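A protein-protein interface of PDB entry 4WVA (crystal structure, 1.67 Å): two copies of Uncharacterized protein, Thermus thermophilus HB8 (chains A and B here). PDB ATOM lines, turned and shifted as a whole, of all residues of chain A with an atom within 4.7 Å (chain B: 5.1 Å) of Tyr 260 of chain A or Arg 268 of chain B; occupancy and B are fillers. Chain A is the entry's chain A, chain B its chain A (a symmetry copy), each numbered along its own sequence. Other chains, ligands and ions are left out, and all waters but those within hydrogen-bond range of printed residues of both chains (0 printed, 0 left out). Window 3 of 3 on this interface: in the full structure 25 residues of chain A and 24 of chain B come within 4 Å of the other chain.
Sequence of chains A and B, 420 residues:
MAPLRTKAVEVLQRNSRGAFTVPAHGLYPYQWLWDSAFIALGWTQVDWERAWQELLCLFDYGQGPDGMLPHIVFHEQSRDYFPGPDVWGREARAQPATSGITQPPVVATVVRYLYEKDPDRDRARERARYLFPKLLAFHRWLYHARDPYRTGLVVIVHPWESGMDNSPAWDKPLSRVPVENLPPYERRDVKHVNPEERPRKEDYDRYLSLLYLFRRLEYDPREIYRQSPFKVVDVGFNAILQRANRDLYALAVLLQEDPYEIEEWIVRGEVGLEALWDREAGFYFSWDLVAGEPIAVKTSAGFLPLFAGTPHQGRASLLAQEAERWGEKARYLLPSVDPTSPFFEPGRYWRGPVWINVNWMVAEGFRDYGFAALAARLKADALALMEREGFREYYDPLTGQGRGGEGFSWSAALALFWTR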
ATOM      1  N   ASP A 258      16.859  33.967  15.217  1.00  0.00           N
ATOM      2  CA  ASP A 258      18.042  33.096  15.311  1.00  0.00           C
ATOM      3  C   ASP A 258      17.542  31.643  15.262  1.00  0.00           C
ATOM      4  O   ASP A 258      16.785  31.233  16.121  1.00  0.00           O
ATOM      5  CB  ASP A 258      18.823  33.399  16.607  1.00  0.00           C
ATOM      6  CG  ASP A 258      20.067  32.540  16.774  1.00  0.00           C
ATOM      7  OD1 ASP A 258      21.178  33.068  17.072  1.00  0.00           O
ATOM      8  OD2 ASP A 258      19.948  31.319  16.621  1.00  0.00           O
ATOM      9  N   PRO A 259      17.938  30.868  14.230  1.00  0.00           N
ATOM     10  CA  PRO A 259      17.450  29.494  14.108  1.00  0.00           C
ATOM     11  C   PRO A 259      18.423  28.420  14.607  1.00  0.00           C
ATOM     12  O   PRO A 259      18.281  27.262  14.232  1.00  0.00           O
ATOM     13  CB  PRO A 259      17.276  29.330  12.585  1.00  0.00           C
ATOM     14  CG  PRO A 259      18.228  30.302  11.982  1.00  0.00           C
ATOM     15  CD  PRO A 259      18.736  31.239  13.048  1.00  0.00           C
ATOM     16  N   TYR A 260      19.403  28.790  15.435  1.00  0.00           N
ATOM     17  CA  TYR A 260      20.474  27.865  15.822  1.00  0.00           C
ATOM     18  C   TYR A 260      19.870  26.602  16.439  1.00  0.00           C
ATOM     19  O   TYR A 260      20.298  25.497  16.111  1.00  0.00           O
ATOM     20  CB  TYR A 260      21.432  28.562  16.812  1.00  0.00           C
ATOM     21  CG  TYR A 260      22.788  27.930  17.015  1.00  0.00           C
ATOM     22  CD1 TYR A 260      23.106  27.283  18.215  1.00  0.00           C
ATOM     23  CD2 TYR A 260      23.786  28.045  16.056  1.00  0.00           C
ATOM     24  CE1 TYR A 260      24.366  26.742  18.426  1.00  0.00           C
ATOM     25  CE2 TYR A 260      25.046  27.510  16.261  1.00  0.00           C
ATOM     26  CZ  TYR A 260      25.332  26.858  17.446  1.00  0.00           C
ATOM     27  OH  TYR A 260      26.589  26.319  17.643  1.00  0.00           O
ATOM     28  N   GLU A 261      18.864  26.790  17.289  1.00  0.00           N
ATOM     29  CA  GLU A 261      18.159  25.701  17.983  1.00  0.00           C
ATOM     30  C   GLU A 261      17.519  24.736  16.974  1.00  0.00           C
ATOM     31  O   GLU A 261      17.642  23.517  17.067  1.00  0.00           O
ATOM     32  CB  GLU A 261      17.087  26.296  18.877  1.00  0.00           C
ATOM     33  CG  GLU A 261      16.467  25.327  19.871  1.00  0.00           C
ATOM     34  CD  GLU A 261      15.520  25.992  20.853  1.00  0.00           C
ATOM     35  OE1 GLU A 261      15.072  25.304  21.794  1.00  0.00           O
ATOM     36  OE2 GLU A 261      15.187  27.189  20.696  1.00  0.00           O
ATOM     37  N   ILE A 262      16.851  25.324  15.997  1.00  0.00           N
ATOM     38  CA  ILE A 262      16.157  24.560  14.952  1.00  0.00           C
ATOM     39  C   ILE A 262      17.162  23.771  14.098  1.00  0.00           C
ATOM     40  O   ILE A 262      16.905  22.636  13.707  1.00  0.00           O
ATOM     41  CB  ILE A 262      15.335  25.493  14.041  1.00  0.00           C
ATOM     42  CG1 ILE A 262      14.352  26.350  14.843  1.00  0.00           C
ATOM     43  CG2 ILE A 262      14.550  24.675  13.021  1.00  0.00           C
ATOM     44  CD1 ILE A 262      13.821  27.533  14.057  1.00  0.00           C
ATOM     45  N   GLU A 263      18.320  24.371  13.812  1.00  0.00           N
ATOM     46  CA  GLU A 263      19.347  23.683  13.049  1.00  0.00           C
ATOM     47  C   GLU A 263      19.755  22.362  13.728  1.00  0.00           C
ATOM     48  O   GLU A 263      19.948  21.351  13.056  1.00  0.00           O
ATOM     49  CB  GLU A 263      20.584  24.566  12.859  1.00  0.00           C
ATOM     50  CG  GLU A 263      20.345  25.834  12.048  1.00  0.00           C
ATOM     51  CD  GLU A 263      21.401  26.894  12.291  1.00  0.00           C
ATOM     52  OE1 GLU A 263      22.511  26.559  12.759  1.00  0.00           O
ATOM     53  OE2 GLU A 263      21.111  28.071  12.029  1.00  0.00           O
ATOM     54  N   GLU A 264      19.884  22.383  15.049  1.00  0.00           N
ATOM     55  CA  GLU A 264      20.228  21.160  15.777  1.00  0.00           C
ATOM     56  C   GLU A 264      19.134  20.113  15.627  1.00  0.00           C
ATOM     57  O   GLU A 264      19.432  18.938  15.396  1.00  0.00           O
ATOM     58  CB  GLU A 264      20.502  21.440  17.254  1.00  0.00           C
ATOM     59  CG  GLU A 264      21.390  22.653  17.463  1.00  0.00           C
ATOM     60  CD  GLU A 264      22.282  22.574  18.680  1.00  0.00           C
ATOM     61  OE1 GLU A 264      22.027  21.728  19.570  1.00  0.00           O
ATOM     62  OE2 GLU A 264      23.250  23.373  18.731  1.00  0.00           O
ATOM     63  N   TYR B 149      22.857  36.071  13.035  1.00  0.00           N
ATOM     64  CA  TYR B 149      21.796  35.214  13.599  1.00  0.00           C
ATOM     65  C   TYR B 149      22.141  33.723  13.519  1.00  0.00           C
ATOM     66  O   TYR B 149      21.272  32.883  13.791  1.00  0.00           O
ATOM     67  CB  TYR B 149      20.454  35.477  12.902  1.00  0.00           C
ATOM     68  CG  TYR B 149      19.867  36.856  13.165  1.00  0.00           C
ATOM     69  CD1 TYR B 149      19.310  37.167  14.406  1.00  0.00           C
ATOM     70  CD2 TYR B 149      19.846  37.832  12.167  1.00  0.00           C
ATOM     71  CE1 TYR B 149      18.765  38.423  14.652  1.00  0.00           C
ATOM     72  CE2 TYR B 149      19.303  39.092  12.400  1.00  0.00           C
ATOM     73  CZ  TYR B 149      18.765  39.378  13.651  1.00  0.00           C
ATOM     74  OH  TYR B 149      18.226  40.619  13.894  1.00  0.00           O
ATOM     75  N   ARG B 150      23.389  33.389  13.160  1.00  0.00           N
ATOM     76  CA  ARG B 150      23.902  32.015  13.209  1.00  0.00           C
ATOM     77  C   ARG B 150      23.077  31.058  12.338  1.00  0.00           C
ATOM     78  O   ARG B 150      22.822  29.894  12.706  1.00  0.00           O
ATOM     79  CB  ARG B 150      23.922  31.521  14.654  1.00  0.00           C
ATOM     80  CG  ARG B 150      24.701  32.430  15.587  1.00  0.00           C
ATOM     81  CD  ARG B 150      24.862  31.768  16.937  1.00  0.00           C
ATOM     82  NE  ARG B 150      23.575  31.636  17.613  1.00  0.00           N
ATOM     83  CZ  ARG B 150      23.370  30.912  18.711  1.00  0.00           C
ATOM     84  NH1 ARG B 150      24.372  30.239  19.272  1.00  0.00           N
ATOM     85  NH2 ARG B 150      22.151  30.847  19.238  1.00  0.00           N
ATOM     86  N   THR B 151      22.678  31.554  11.183  1.00  0.00           N
ATOM     87  CA  THR B 151      21.809  30.825  10.278  1.00  0.00           C
ATOM     88  C   THR B 151      22.518  29.784   9.433  1.00  0.00           C
ATOM     89  O   THR B 151      21.868  28.859   8.924  1.00  0.00           O
ATOM     90  CB  THR B 151      21.057  31.763   9.298  1.00  0.00           C
ATOM     91  OG1 THR B 151      21.974  32.352   8.356  1.00  0.00           O
ATOM     92  CG2 THR B 151      20.302  32.853  10.039  1.00  0.00           C
ATOM     93  N   GLY B 152      23.824  29.952   9.218  1.00  0.00           N
ATOM     94  CA  GLY B 152      24.548  29.142   8.233  1.00  0.00           C
ATOM     95  C   GLY B 152      24.577  29.740   6.833  1.00  0.00           C
ATOM     96  O   GLY B 152      25.307  29.237   5.951  1.00  0.00           O
ATOM     97  N   GLU B 263      33.825  22.495  10.087  1.00  0.00           N
ATOM     98  CA  GLU B 263      32.778  21.490  10.071  1.00  0.00           C
ATOM     99  C   GLU B 263      31.410  22.103  10.424  1.00  0.00           C
ATOM    100  O   GLU B 263      30.400  21.766   9.810  1.00  0.00           O
ATOM    101  CB  GLU B 263      33.093  20.345  11.039  1.00  0.00           C
ATOM    102  CG  GLU B 263      34.342  19.544  10.697  1.00  0.00           C
ATOM    103  CD  GLU B 263      34.896  18.783  11.885  1.00  0.00           C
ATOM    104  OE1 GLU B 263      34.149  18.537  12.858  1.00  0.00           O
ATOM    105  OE2 GLU B 263      36.087  18.444  11.851  1.00  0.00           O
ATOM    106  N   GLU B 264      31.389  22.993  11.408  1.00  0.00           N
ATOM    107  CA  GLU B 264      30.136  23.657  11.779  1.00  0.00           C
ATOM    108  C   GLU B 264      29.612  24.506  10.632  1.00  0.00           C
ATOM    109  O   GLU B 264      28.414  24.475  10.339  1.00  0.00           O
ATOM    110  CB  GLU B 264      30.298  24.501  13.041  1.00  0.00           C
ATOM    111  CG  GLU B 264      31.057  23.775  14.137  1.00  0.00           C
ATOM    112  CD  GLU B 264      30.639  24.147  15.541  1.00  0.00           C
ATOM    113  OE1 GLU B 264      29.973  25.194  15.723  1.00  0.00           O
ATOM    114  OE2 GLU B 264      30.986  23.369  16.464  1.00  0.00           O
ATOM    115  N   TRP B 265      30.502  25.219   9.939  1.00  0.00           N
ATOM    116  CA  TRP B 265      30.064  26.025   8.803  1.00  0.00           C
ATOM    117  C   TRP B 265      29.445  25.140   7.724  1.00  0.00           C
ATOM    118  O   TRP B 265      28.439  25.497   7.089  1.00  0.00           O
ATOM    119  CB  TRP B 265      31.213  26.825   8.178  1.00  0.00           C
ATOM    120  CG  TRP B 265      31.910  27.774   9.122  1.00  0.00           C
ATOM    121  CD1 TRP B 265      31.388  28.379  10.220  1.00  0.00           C
ATOM    122  CD2 TRP B 265      33.258  28.252   9.005  1.00  0.00           C
ATOM    123  NE1 TRP B 265      32.323  29.199  10.801  1.00  0.00           N
ATOM    124  CE2 TRP B 265      33.481  29.139  10.074  1.00  0.00           C
ATOM    125  CE3 TRP B 265      34.296  28.019   8.100  1.00  0.00           C
ATOM    126  CZ2 TRP B 265      34.709  29.766  10.276  1.00  0.00           C
ATOM    127  CZ3 TRP B 265      35.504  28.651   8.300  1.00  0.00           C
ATOM    128  CH2 TRP B 265      35.700  29.513   9.384  1.00  0.00           C
ATOM    129  N   ILE B 266      30.070  24.003   7.489  1.00  0.00           N
ATOM    130  CA  ILE B 266      29.614  23.082   6.449  1.00  0.00           C
ATOM    131  C   ILE B 266      28.212  22.530   6.774  1.00  0.00           C
ATOM    132  O   ILE B 266      27.320  22.510   5.927  1.00  0.00           O
ATOM    133  CB  ILE B 266      30.628  21.927   6.289  1.00  0.00           C
ATOM    134  CG1 ILE B 266      31.930  22.455   5.665  1.00  0.00           C
ATOM    135  CG2 ILE B 266      30.029  20.815   5.448  1.00  0.00           C
ATOM    136  CD1 ILE B 266      33.073  21.470   5.643  1.00  0.00           C
ATOM    137  N   VAL B 267      28.042  22.058   7.998  1.00  0.00           N
ATOM    138  CA  VAL B 267      26.812  21.393   8.387  1.00  0.00           C
ATOM    139  C   VAL B 267      25.660  22.385   8.435  1.00  0.00           C
ATOM    140  O   VAL B 267      24.606  22.125   7.879  1.00  0.00           O
ATOM    141  CB  VAL B 267      27.001  20.652   9.717  1.00  0.00           C
ATOM    142  CG1 VAL B 267      25.689  20.106  10.250  1.00  0.00           C
ATOM    143  CG2 VAL B 267      28.009  19.537   9.498  1.00  0.00           C
ATOM    144  N   ARG B 268      25.892  23.542   9.042  1.00  0.00           N
ATOM    145  CA  ARG B 268      24.854  24.579   9.091  1.00  0.00           C
ATOM    146  C   ARG B 268      24.596  25.190   7.718  1.00  0.00           C
ATOM    147  O   ARG B 268      23.465  25.534   7.393  1.00  0.00           O
ATOM    148  CB  ARG B 268      25.191  25.626  10.160  1.00  0.00           C
ATOM    149  CG  ARG B 268      25.268  24.984  11.532  1.00  0.00           C
ATOM    150  CD  ARG B 268      25.647  25.894  12.685  1.00  0.00           C
ATOM    151  NE  ARG B 268      25.928  25.083  13.892  1.00  0.00           N
ATOM    152  CZ  ARG B 268      25.017  24.590  14.739  1.00  0.00           C
ATOM    153  NH1 ARG B 268      23.715  24.818  14.581  1.00  0.00           N
ATOM    154  NH2 ARG B 268      25.411  23.877  15.791  1.00  0.00           N
ATOM    155  N   GLY B 269      25.636  25.283   6.888  1.00  0.00           N
ATOM    156  CA  GLY B 269      25.475  25.773   5.540  1.00  0.00           C
ATOM    157  C   GLY B 269      24.705  24.862   4.625  1.00  0.00           C
ATOM    158  O   GLY B 269      24.024  25.328   3.701  1.00  0.00           O
ATOM    159  N   GLU B 270      24.794  23.556   4.867  1.00  0.00           N
ATOM    160  CA  GLU B 270      24.060  22.605   4.069  1.00  0.00           C
ATOM    161  C   GLU B 270      22.568  22.770   4.343  1.00  0.00           C
ATOM    162  O   GLU B 270      21.740  22.713   3.430  1.00  0.00           O
ATOM    163  CB  GLU B 270      24.502  21.185   4.420  1.00  0.00           C
ATOM    164  CG  GLU B 270      23.875  20.142   3.521  1.00  0.00           C
ATOM    165  CD  GLU B 270      24.561  18.807   3.623  1.00  0.00           C
ATOM    166  OE1 GLU B 270      25.434  18.650   4.506  1.00  0.00           O
ATOM    167  OE2 GLU B 270      24.212  17.916   2.818  1.00  0.00           O
ATOM    168  N   VAL B 271      22.227  22.962   5.617  1.00  0.00           N
ATOM    169  CA  VAL B 271      20.835  23.199   5.996  1.00  0.00           C
ATOM    170  C   VAL B 271      20.334  24.475   5.314  1.00  0.00           C
ATOM    171  O   VAL B 271      19.291  24.467   4.692  1.00  0.00           O
ATOM    172  CB  VAL B 271      20.650  23.338   7.508  1.00  0.00           C
ATOM    173  CG1 VAL B 271      19.222  23.759   7.832  1.00  0.00           C
ATOM    174  CG2 VAL B 271      21.006  22.036   8.203  1.00  0.00           C
ATOM    175  N   GLY B 272      21.112  25.546   5.420  1.00  0.00           N
ATOM    176  CA  GLY B 272      20.715  26.841   4.852  1.00  0.00           C
ATOM    177  C   GLY B 272      20.555  26.805   3.346  1.00  0.00           C
ATOM    178  O   GLY B 272      19.569  27.275   2.793  1.00  0.00           O
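OD1 of Asp 258 of chain A is in salt-bridge range of NE of Arg 150 of chain B.
The side-chain hydroxyl (OH) of Tyr 260 of chain A is in hydrogen-bond range of the guanidinium group (NH2) of Arg 268 of chain B (3.3 Å).
The side-chain carboxylate (OE2) of Glu 263 of chain A lies close to the backbone carbonyl oxygen (O) of Arg 150 of chain B, at 2.6 Å.
The side-chain carboxylate (OE1) of Glu 263 of chain A lies within salt-bridge range of the guanidinium group (NH1) of Arg 268 of chain B.
The side-chain carboxylate of Glu 264 of chain A is in salt-bridge range of the guanidinium group of Arg 268 of chain B, 3.7 Å away.
OD1 of Asp 258 of chain A lies close to O of Tyr 149 of chain B (3.3 Å).
The side-chain carboxylate of Glu 263 of chain A sits close to the backbone carbonyl oxygen of Thr 151 of chain B, 3.3 Å away.
N of Tyr 260 of chain A is in hydrogen-bond range of OD2 of Asp 258 of chain A, 2.8 Å away.
O of Tyr 149 of chain B touches CD of Pro 259 of chain A (3.1 Å).
Pro 259 of chain A touches Thr 151 of chain B (CD to CG2, 3.8 Å).
Tyr 260 of chain A touches Arg 150 of chain B (CD1 to NH1, 3.4 Å).
Of the printed residues of chain B, Asp 258 of chain A touches Tyr 149 (3.2 Å) and Arg 150 (2.8 Å).
Of chain B, only Arg 150 (3.4 Å) and Arg 268 (3.3 Å) come within 4 Å of Tyr 260 of chain A.
Of the printed residues of chain B, Glu 263 of chain A touches Arg 150 (2.6 Å), Thr 151 (3.3 Å) and Arg 268 (2.8 Å).
Printed residues of chain B within 4 Å of Glu 264 of chain A: Arg 268.
Printed residues of chain A within 4 Å of Arg 150 of chain B: Asp 258, Tyr 260 and Glu 263.
Of the printed residues of chain A, Thr 151 of chain B touches Pro 259 and Glu 263.
Arg 268 of chain B touches just these residues of chain A: Tyr 260, Glu 263 and Glu 264.
Glu 270 of chain B touches none of the printed residues of chain A.
The nearest residue of chain B that does not touch Tyr 260 of chain A is Glu 264 of chain B (4.1 Å).
The nearest printed residue of chain A that does not touch Arg 268 of chain B is Glu 261 of chain A (5.9 Å).
Printed residues of chain A that touch a printed residue of chain B: Asp 258, Pro 259, Tyr 260, Glu 263 and Glu 264.
Hydrophobic or aromatic side chains of chain A that line the printed part of chain B: Pro 259 and Tyr 260.
Along chain A the printed residues that touch a printed residue of chain B span positions 258 to 264.
Among the printed residues, 10 pairs touch across the chains.
Among the printed residues, Asp or Glu carboxylates within 4 Å of a Lys or Arg side-chain nitrogen of the other chain: Asp 258 of chain A with Arg 150 of chain B, Glu 263 of chain A with Arg 268 of chain B and Glu 264 of chain A with Arg 268 of chain B.
2 positions are printed for both chains.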
